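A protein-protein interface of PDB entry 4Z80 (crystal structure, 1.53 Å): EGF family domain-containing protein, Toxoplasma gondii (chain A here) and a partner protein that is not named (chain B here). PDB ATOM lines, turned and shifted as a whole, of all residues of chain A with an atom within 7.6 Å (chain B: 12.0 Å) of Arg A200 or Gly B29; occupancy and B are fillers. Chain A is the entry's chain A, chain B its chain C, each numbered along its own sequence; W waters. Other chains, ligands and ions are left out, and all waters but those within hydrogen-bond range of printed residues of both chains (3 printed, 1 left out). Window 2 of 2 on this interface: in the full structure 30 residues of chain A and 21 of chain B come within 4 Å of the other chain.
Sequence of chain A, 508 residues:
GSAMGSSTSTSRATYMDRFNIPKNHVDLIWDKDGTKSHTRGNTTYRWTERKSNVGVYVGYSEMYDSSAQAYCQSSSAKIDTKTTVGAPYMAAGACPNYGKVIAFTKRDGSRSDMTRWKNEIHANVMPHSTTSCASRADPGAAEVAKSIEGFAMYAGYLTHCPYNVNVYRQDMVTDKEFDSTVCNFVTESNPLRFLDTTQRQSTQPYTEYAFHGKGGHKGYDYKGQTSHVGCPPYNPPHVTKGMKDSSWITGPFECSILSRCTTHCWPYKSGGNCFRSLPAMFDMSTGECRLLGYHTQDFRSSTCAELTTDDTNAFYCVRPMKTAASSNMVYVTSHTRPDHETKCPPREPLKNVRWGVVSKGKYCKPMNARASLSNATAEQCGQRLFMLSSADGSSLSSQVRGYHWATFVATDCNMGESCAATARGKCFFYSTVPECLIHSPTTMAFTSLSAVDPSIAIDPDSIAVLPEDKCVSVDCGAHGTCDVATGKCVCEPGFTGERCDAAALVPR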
ATOM      1  N   ASP A 196       3.090  -5.754  19.017  1.00  0.00           N
ATOM      2  CA  ASP A 196       2.486  -4.721  18.185  1.00  0.00           C
ATOM      3  C   ASP A 196       1.172  -4.255  18.793  1.00  0.00           C
ATOM      4  O   ASP A 196       0.142  -4.913  18.657  1.00  0.00           O
ATOM      5  CB  ASP A 196       2.256  -5.238  16.767  1.00  0.00           C
ATOM      6  CG  ASP A 196       1.863  -4.133  15.804  1.00  0.00           C
ATOM      7  OD1 ASP A 196       1.671  -2.985  16.262  1.00  0.00           O
ATOM      8  OD2 ASP A 196       1.746  -4.412  14.593  1.00  0.00           O
ATOM      9  N   THR A 197       1.221  -3.111  19.456  1.00  0.00           N
ATOM     10  CA  THR A 197       0.072  -2.599  20.188  1.00  0.00           C
ATOM     11  C   THR A 197      -0.924  -1.913  19.256  1.00  0.00           C
ATOM     12  O   THR A 197      -2.028  -1.555  19.673  1.00  0.00           O
ATOM     13  CB  THR A 197       0.526  -1.621  21.282  1.00  0.00           C
ATOM     14  OG1 THR A 197       1.282  -0.558  20.688  1.00  0.00           O
ATOM     15  CG2 THR A 197       1.397  -2.351  22.306  1.00  0.00           C
ATOM     16  N   THR A 198      -0.537  -1.743  17.994  1.00  0.00           N
ATOM     17  CA  THR A 198      -1.434  -1.179  16.990  1.00  0.00           C
ATOM     18  C   THR A 198      -2.396  -2.244  16.456  1.00  0.00           C
ATOM     19  O   THR A 198      -3.268  -1.944  15.638  1.00  0.00           O
ATOM     20  CB  THR A 198      -0.655  -0.563  15.806  1.00  0.00           C
ATOM     21  OG1 THR A 198      -0.085  -1.603  15.003  1.00  0.00           O
ATOM     22  CG2 THR A 198       0.451   0.363  16.304  1.00  0.00           C
ATOM     23  N   GLN A 199      -2.235  -3.481  16.924  1.00  0.00           N
ATOM     24  CA  GLN A 199      -3.106  -4.585  16.532  1.00  0.00           C
ATOM     25  C   GLN A 199      -3.589  -5.342  17.765  1.00  0.00           C
ATOM     26  O   GLN A 199      -3.084  -6.420  18.087  1.00  0.00           O
ATOM     27  CB  GLN A 199      -2.377  -5.533  15.572  1.00  0.00           C
ATOM     28  CG  GLN A 199      -1.890  -4.860  14.294  1.00  0.00           C
ATOM     29  CD  GLN A 199      -1.057  -5.784  13.417  1.00  0.00           C
ATOM     30  OE1 GLN A 199      -0.693  -6.887  13.828  1.00  0.00           O
ATOM     31  NE2 GLN A 199      -0.749  -5.334  12.204  1.00  0.00           N
ATOM     32  N   ARG A 200      -4.569  -4.770  18.454  1.00  0.00           N
ATOM     33  CA  ARG A 200      -5.115  -5.383  19.658  1.00  0.00           C
ATOM     34  C   ARG A 200      -5.927  -6.630  19.320  1.00  0.00           C
ATOM     35  O   ARG A 200      -6.347  -6.818  18.177  1.00  0.00           O
ATOM     36  CB  ARG A 200      -5.991  -4.385  20.420  1.00  0.00           C
ATOM     37  CG  ARG A 200      -5.252  -3.152  20.923  1.00  0.00           C
ATOM     38  CD  ARG A 200      -6.129  -2.337  21.860  1.00  0.00           C
ATOM     39  NE  ARG A 200      -5.420  -1.972  23.086  1.00  0.00           N
ATOM     40  CZ  ARG A 200      -5.959  -1.962  24.304  1.00  0.00           C
ATOM     41  NH1 ARG A 200      -7.231  -2.299  24.491  1.00  0.00           N
ATOM     42  NH2 ARG A 200      -5.217  -1.613  25.347  1.00  0.00           N
ATOM     43  N   GLN A 201      -6.136  -7.477  20.324  1.00  0.00           N
ATOM     44  CA  GLN A 201      -6.941  -8.684  20.171  1.00  0.00           C
ATOM     45  C   GLN A 201      -7.964  -8.798  21.295  1.00  0.00           C
ATOM     46  O   GLN A 201      -7.896  -8.070  22.286  1.00  0.00           O
ATOM     47  CB  GLN A 201      -6.055  -9.928  20.157  1.00  0.00           C
ATOM     48  CG  GLN A 201      -5.064  -9.983  19.012  1.00  0.00           C
ATOM     49  CD  GLN A 201      -4.137 -11.175  19.120  1.00  0.00           C
ATOM     50  OE1 GLN A 201      -4.402 -12.115  19.872  1.00  0.00           O
ATOM     51  NE2 GLN A 201      -3.040 -11.142  18.374  1.00  0.00           N
ATOM     52  N   SER A 202      -8.908  -9.720  21.135  1.00  0.00           N
ATOM     53  CA  SER A 202      -9.901  -9.986  22.166  1.00  0.00           C
ATOM     54  C   SER A 202      -9.230 -10.573  23.407  1.00  0.00           C
ATOM     55  O   SER A 202      -9.684 -10.358  24.533  1.00  0.00           O
ATOM     56  CB  SER A 202     -10.976 -10.943  21.644  1.00  0.00           C
ATOM     57  OG  SER A 202     -10.617 -12.293  21.885  1.00  0.00           O
ATOM     58  N   THR A 203      -8.143 -11.309  23.189  1.00  0.00           N
ATOM     59  CA  THR A 203      -7.423 -11.973  24.272  1.00  0.00           C
ATOM     60  C   THR A 203      -6.435 -11.032  24.964  1.00  0.00           C
ATOM     61  O   THR A 203      -6.275 -11.085  26.183  1.00  0.00           O
ATOM     62  CB  THR A 203      -6.652 -13.208  23.755  1.00  0.00           C
ATOM     63  OG1 THR A 203      -7.522 -14.024  22.959  1.00  0.00           O
ATOM     64  CG2 THR A 203      -6.106 -14.034  24.918  1.00  0.00           C
ATOM     65  N   GLN A 204      -5.776 -10.178  24.185  1.00  0.00           N
ATOM     66  CA  GLN A 204      -4.736  -9.299  24.722  1.00  0.00           C
ATOM     67  C   GLN A 204      -4.597  -8.026  23.878  1.00  0.00           C
ATOM     68  O   GLN A 204      -4.998  -8.005  22.715  1.00  0.00           O
ATOM     69  CB  GLN A 204      -3.405 -10.053  24.786  1.00  0.00           C
ATOM     70  CG  GLN A 204      -2.684 -10.148  23.444  1.00  0.00           C
ATOM     71  CD  GLN A 204      -1.958 -11.464  23.239  1.00  0.00           C
ATOM     72  OE1 GLN A 204      -2.257 -12.468  23.887  1.00  0.00           O
ATOM     73  NE2 GLN A 204      -1.000 -11.468  22.319  1.00  0.00           N
ATOM     74  N   PRO A 205      -4.023  -6.960  24.462  1.00  0.00           N
ATOM     75  CA  PRO A 205      -3.964  -5.646  23.804  1.00  0.00           C
ATOM     76  C   PRO A 205      -2.819  -5.483  22.797  1.00  0.00           C
ATOM     77  O   PRO A 205      -2.315  -4.373  22.613  1.00  0.00           O
ATOM     78  CB  PRO A 205      -3.783  -4.688  24.986  1.00  0.00           C
ATOM     79  CG  PRO A 205      -2.998  -5.478  25.964  1.00  0.00           C
ATOM     80  CD  PRO A 205      -3.499  -6.895  25.841  1.00  0.00           C
ATOM     81  N   TYR A 206      -2.427  -6.570  22.143  1.00  0.00           N
ATOM     82  CA  TYR A 206      -1.364  -6.514  21.146  1.00  0.00           C
ATOM     83  C   TYR A 206      -1.297  -7.819  20.374  1.00  0.00           C
ATOM     84  O   TYR A 206      -1.875  -8.823  20.789  1.00  0.00           O
ATOM     85  CB  TYR A 206      -0.008  -6.238  21.806  1.00  0.00           C
ATOM     86  CG  TYR A 206       0.355  -7.251  22.867  1.00  0.00           C
ATOM     87  CD1 TYR A 206       1.009  -8.431  22.536  1.00  0.00           C
ATOM     88  CD2 TYR A 206       0.029  -7.035  24.198  1.00  0.00           C
ATOM     89  CE1 TYR A 206       1.335  -9.363  23.503  1.00  0.00           C
ATOM     90  CE2 TYR A 206       0.351  -7.958  25.173  1.00  0.00           C
ATOM     91  CZ  TYR A 206       1.006  -9.122  24.821  1.00  0.00           C
ATOM     92  OH  TYR A 206       1.328 -10.042  25.790  1.00  0.00           O
ATOM     93  N   THR A 207      -0.588  -7.794  19.251  1.00  0.00           N
ATOM     94  CA  THR A 207      -0.267  -9.012  18.523  1.00  0.00           C
ATOM     95  C   THR A 207       1.232  -9.268  18.669  1.00  0.00           C
ATOM     96  O   THR A 207       2.043  -8.353  18.516  1.00  0.00           O
ATOM     97  CB  THR A 207      -0.651  -8.918  17.036  1.00  0.00           C
ATOM     98  OG1 THR A 207      -2.059  -8.671  16.920  1.00  0.00           O
ATOM     99  CG2 THR A 207      -0.319 -10.217  16.312  1.00  0.00           C
ATOM    100  N   SER A 227      -1.091 -10.679  34.229  1.00  0.00           N
ATOM    101  CA  SER A 227      -1.573  -9.790  33.180  1.00  0.00           C
ATOM    102  C   SER A 227      -0.675  -8.550  33.079  1.00  0.00           C
ATOM    103  O   SER A 227      -0.830  -7.735  32.170  1.00  0.00           O
ATOM    104  CB  SER A 227      -3.033  -9.390  33.434  1.00  0.00           C
ATOM    105  OG  SER A 227      -3.171  -8.735  34.676  1.00  0.00           O
ATOM    106  N   VAL A 229       2.459  -7.448  31.875  1.00  0.00           N
ATOM    107  CA  VAL A 229       3.387  -8.020  30.896  1.00  0.00           C
ATOM    108  C   VAL A 229       4.848  -7.824  31.286  1.00  0.00           C
ATOM    109  O   VAL A 229       5.319  -6.700  31.465  1.00  0.00           O
ATOM    110  CB  VAL A 229       3.156  -7.414  29.498  1.00  0.00           C
ATOM    111  CG1 VAL A 229       4.140  -7.979  28.486  1.00  0.00           C
ATOM    112  CG2 VAL A 229       1.740  -7.683  29.038  1.00  0.00           C
ATOM    113  N   SER B  18      10.165   4.374  31.216  1.00  0.00           N
ATOM    114  CA  SER B  18       8.860   4.127  30.634  1.00  0.00           C
ATOM    115  C   SER B  18       7.731   4.478  31.587  1.00  0.00           C
ATOM    116  O   SER B  18       7.858   4.323  32.799  1.00  0.00           O
ATOM    117  CB  SER B  18       8.737   2.658  30.226  1.00  0.00           C
ATOM    118  OG  SER B  18       7.449   2.367  29.711  1.00  0.00           O
ATOM    119  N   GLY B  19       6.627   4.952  31.025  1.00  0.00           N
ATOM    120  CA  GLY B  19       5.427   5.148  31.810  1.00  0.00           C
ATOM    121  C   GLY B  19       4.769   3.822  32.159  1.00  0.00           C
ATOM    122  O   GLY B  19       3.960   3.757  33.081  1.00  0.00           O
ATOM    123  N   CYS B  20       5.122   2.766  31.424  1.00  0.00           N
ATOM    124  CA  CYS B  20       4.507   1.448  31.600  1.00  0.00           C
ATOM    125  C   CYS B  20       5.533   0.316  31.701  1.00  0.00           C
ATOM    126  O   CYS B  20       5.558  -0.578  30.850  1.00  0.00           O
ATOM    127  CB  CYS B  20       3.554   1.157  30.440  1.00  0.00           C
ATOM    128  SG  CYS B  20       2.118   2.259  30.362  1.00  0.00           S
ATOM    129  N   PRO B  21       6.372   0.342  32.745  1.00  0.00           N
ATOM    130  CA  PRO B  21       7.362  -0.724  32.929  1.00  0.00           C
ATOM    131  C   PRO B  21       6.696  -2.050  33.283  1.00  0.00           C
ATOM    132  O   PRO B  21       5.561  -2.041  33.749  1.00  0.00           O
ATOM    133  CB  PRO B  21       8.214  -0.215  34.089  1.00  0.00           C
ATOM    134  CG  PRO B  21       7.280   0.661  34.877  1.00  0.00           C
ATOM    135  CD  PRO B  21       6.398   1.319  33.850  1.00  0.00           C
ATOM    136  N   PRO B  22       7.409  -3.175  33.104  1.00  0.00           N
ATOM    137  CA  PRO B  22       8.804  -3.252  32.660  1.00  0.00           C
ATOM    138  C   PRO B  22       9.013  -3.442  31.154  1.00  0.00           C
ATOM    139  O   PRO B  22      10.170  -3.393  30.722  1.00  0.00           O
ATOM    140  CB  PRO B  22       9.322  -4.475  33.416  1.00  0.00           C
ATOM    141  CG  PRO B  22       8.140  -5.372  33.498  1.00  0.00           C
ATOM    142  CD  PRO B  22       6.948  -4.457  33.668  1.00  0.00           C
ATOM    143  N   MET B  23       7.951  -3.668  30.383  1.00  0.00           N
ATOM    144  CA  MET B  23       8.099  -3.938  28.954  1.00  0.00           C
ATOM    145  C   MET B  23       7.458  -2.876  28.063  1.00  0.00           C
ATOM    146  O   MET B  23       7.688  -2.869  26.853  1.00  0.00           O
ATOM    147  CB  MET B  23       7.509  -5.307  28.619  1.00  0.00           C
ATOM    148  CG  MET B  23       8.346  -6.471  29.125  1.00  0.00           C
ATOM    149  SD  MET B  23       9.732  -6.865  28.035  1.00  0.00           S
ATOM    150  CE  MET B  23       8.848  -7.548  26.629  1.00  0.00           C
ATOM    151  N   GLY B  24       6.657  -1.994  28.655  1.00  0.00           N
ATOM    152  CA  GLY B  24       6.014  -0.924  27.907  1.00  0.00           C
ATOM    153  C   GLY B  24       4.509  -1.091  27.740  1.00  0.00           C
ATOM    154  O   GLY B  24       3.878  -0.331  27.006  1.00  0.00           O
ATOM    155  N   ILE B  25       3.939  -2.084  28.417  1.00  0.00           N
ATOM    156  CA  ILE B  25       2.486  -2.275  28.469  1.00  0.00           C
ATOM    157  C   ILE B  25       2.017  -2.132  29.914  1.00  0.00           C
ATOM    158  O   ILE B  25       2.472  -2.859  30.794  1.00  0.00           O
ATOM    159  CB  ILE B  25       2.066  -3.659  27.914  1.00  0.00           C
ATOM    160  CG1 ILE B  25       2.546  -3.815  26.468  1.00  0.00           C
ATOM    161  CG2 ILE B  25       0.550  -3.832  27.985  1.00  0.00           C
ATOM    162  CD1 ILE B  25       2.282  -5.168  25.875  1.00  0.00           C
ATOM    163  N   CYS B  26       1.114  -1.189  30.167  1.00  0.00           N
ATOM    164  CA  CYS B  26       0.670  -0.947  31.538  1.00  0.00           C
ATOM    165  C   CYS B  26      -0.294  -2.042  32.006  1.00  0.00           C
ATOM    166  O   CYS B  26      -0.826  -2.807  31.197  1.00  0.00           O
ATOM    167  CB  CYS B  26       0.026   0.439  31.655  1.00  0.00           C
ATOM    168  SG  CYS B  26       1.219   1.741  32.107  1.00  0.00           S
ATOM    169  N   MET B  27      -0.480  -2.120  33.322  1.00  0.00           N
ATOM    170  CA  MET B  27      -1.346  -3.108  33.959  1.00  0.00           C
ATOM    171  C   MET B  27      -2.727  -3.187  33.291  1.00  0.00           C
ATOM    172  O   MET B  27      -3.345  -4.253  33.268  1.00  0.00           O
ATOM    173  CB  MET B  27      -1.472  -2.761  35.451  1.00  0.00           C
ATOM    174  CG  MET B  27      -2.505  -3.591  36.252  1.00  0.00           C
ATOM    175  SD  MET B  27      -3.499  -2.532  37.315  1.00  0.00           S
ATOM    176  CE  MET B  27      -2.272  -1.920  38.472  1.00  0.00           C
ATOM    177  N   ASP B  28      -3.191  -2.077  32.720  1.00  0.00           N
ATOM    178  CA  ASP B  28      -4.511  -2.027  32.091  1.00  0.00           C
ATOM    179  C   ASP B  28      -4.456  -2.178  30.566  1.00  0.00           C
ATOM    180  O   ASP B  28      -5.449  -1.944  29.876  1.00  0.00           O
ATOM    181  CB  ASP B  28      -5.211  -0.717  32.458  1.00  0.00           C
ATOM    182  CG  ASP B  28      -4.603   0.491  31.773  1.00  0.00           C
ATOM    183  OD1 ASP B  28      -3.402   0.454  31.430  1.00  0.00           O
ATOM    184  OD2 ASP B  28      -5.335   1.488  31.589  1.00  0.00           O
ATOM    185  N   GLY B  29      -3.297  -2.570  30.043  1.00  0.00           N
ATOM    186  CA  GLY B  29      -3.172  -2.890  28.631  1.00  0.00           C
ATOM    187  C   GLY B  29      -2.900  -1.693  27.734  1.00  0.00           C
ATOM    188  O   GLY B  29      -2.698  -1.858  26.531  1.00  0.00           O
ATOM    189  N   THR B  30      -2.904  -0.491  28.304  1.00  0.00           N
ATOM    190  CA  THR B  30      -2.529   0.704  27.550  1.00  0.00           C
ATOM    191  C   THR B  30      -1.007   0.738  27.429  1.00  0.00           C
ATOM    192  O   THR B  30      -0.314  -0.009  28.125  1.00  0.00           O
ATOM    193  CB  THR B  30      -3.032   2.002  28.221  1.00  0.00           C
ATOM    194  OG1 THR B  30      -2.370   2.191  29.479  1.00  0.00           O
ATOM    195  CG2 THR B  30      -4.534   1.948  28.448  1.00  0.00           C
ATOM    196  N   ILE B  31      -0.464   1.675  26.663  1.00  0.00           N
ATOM    197  CA  ILE B  31       0.989   1.840  26.547  1.00  0.00           C
ATOM    198  C   ILE B  31       1.536   3.133  27.034  1.00  0.00           C
ATOM    199  O   ILE B  31       0.841   4.058  27.299  1.00  0.00           O
ATOM    200  CB  ILE B  31       1.505   1.766  25.096  1.00  0.00           C
ATOM    201  CG1 ILE B  31       0.817   2.785  24.255  1.00  0.00           C
ATOM    202  CG2 ILE B  31       1.322   0.420  24.508  1.00  0.00           C
ATOM    203  CD1 ILE B  31       1.679   3.335  23.153  1.00  0.00           C
ATOM    204  N   GLY B  32       2.832   3.143  27.151  1.00  0.00           N
ATOM    205  CA  GLY B  32       3.670   4.291  27.007  1.00  0.00           C
ATOM    206  C   GLY B  32       3.078   5.661  26.956  1.00  0.00           C
ATOM    207  O   GLY B  32       2.183   5.965  26.263  1.00  0.00           O
ATOM    208  N   ASP B  33       3.615   6.478  27.795  1.00  0.00           N
ATOM    209  CA  ASP B  33       4.533   7.468  27.446  1.00  0.00           C
ATOM    210  C   ASP B  33       5.845   6.750  27.521  1.00  0.00           C
ATOM    211  O   ASP B  33       6.205   6.287  28.560  1.00  0.00           O
ATOM    212  CB  ASP B  33       4.491   8.614  28.420  1.00  0.00           C
ATOM    213  CG  ASP B  33       5.407   9.698  28.064  1.00  0.00           C
ATOM    214  OD1 ASP B  33       6.351   9.466  27.322  1.00  0.00           O
ATOM    215  OD2 ASP B  33       5.184  10.822  28.549  1.00  0.00           O
HETATM  216  O   HOH W   1      -2.293  -5.901  34.701  1.00  0.00           O
HETATM  217  O   HOH W   2      -1.834  -5.729  30.304  1.00  0.00           O
HETATM  218  O   HOH W   3       5.023  -4.056  30.639  1.00  0.00           O
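Thr A197 touches just one residue of chain B: Ile B31 (3.5 Å).
No residue of chain B comes within 4 Å of Gln A199.
No residue of chain B comes within 4 Å of Gln A201.
Pro A205 touches just one residue of chain B: Gly B29.
Of the printed residues of chain B, Tyr A206 touches Ile B25.
No residue of chain B comes within 4 Å of Thr A207.
Ser B18 touches none of the printed residues of chain A.
Printed residues of chain A within 4 Å of Ile B25: Tyr A206.
Of chain A, only Arg A200 and Pro A205 come within 4 Å of Gly B29.
Of the printed residues of chain A, Ile B31 touches Thr A197.
Gly B32 touches none of the printed residues of chain A.
The nearest residue of chain A that does not touch Gly B29 is Thr A197 (5.9 Å).
The nearest printed residue of chain A that does not touch Ile B31 is Arg A200 (5.9 Å).
Water W1 bridges O of Met B27 (2.4 Å) and OG of Ser A227 (3.0 Å).
Water W3 lies within hydrogen-bond range of O of Val A229 (2.8 Å), O of Ile B25 (2.8 Å), N of Met B23 (3.0 Å) and N of Gly B24 (3.3 Å).
Water W2 lies within hydrogen-bond range of the backbone carbonyl oxygen of Ser A227 (2.9 Å), the backbone carbonyl oxygen of Cys B26 (3.2 Å) and the backbone NH of Gly B29 (3.5 Å).
O of Gly B29 sits at hydrogen-bond distance from NH2 of Arg A200, at 2.8 Å.
Of the 14 printed residues of chain A, 5 touch a printed residue of chain B.
Hydrophobic or aromatic side chains of chain A that line the printed part of chain B: Pro A205 and Tyr A206.
Of the 16 printed residues of chain B, 6 touch a printed residue of chain A.
Printed residues of chain B that touch a printed residue of chain A: Pro B22, Met B23, Ile B25, Gly B29, Thr B30 and Ile B31.
Hydrophobic or aromatic side chains of chain B within 4 Å of the printed part of chain A: Pro B22, Met B23, Ile B25 and Ile B31.
Among the printed residues, no Asp or Glu carboxylate lies within 4 Å of a Lys or Arg side-chain nitrogen of the other chain.
Among the printed residues, merely in contact across the chains: Thr A197 with Ile B31 (3.5 Å), Arg A200 with Thr B30 (3.9 Å), Pro A205 with Gly B29 (3.4 Å), Tyr A206 with Ile B25 (3.4 Å), Val A229 with Pro B22 (3.5 Å) and Val A229 with Met B23 (3.8 Å).
The backbone NH of Ile B25 is in hydrogen-bond range of the backbone carbonyl oxygen of Cys B20, at 3.3 Å.
The side-chain sulfur of Cys B26 forms a disulfide with the side-chain sulfur of Cys B20, at 2.0 Å.
The side-chain amide nitrogen (NE2) of Gln A204 sits close to the backbone carbonyl oxygen (O) of Tyr A206.
The side-chain carboxylate (OD1) of Asp B28 lies within hydrogen-bond range of the side-chain hydroxyl (OG1) of Thr B30, at 2.8 Å.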
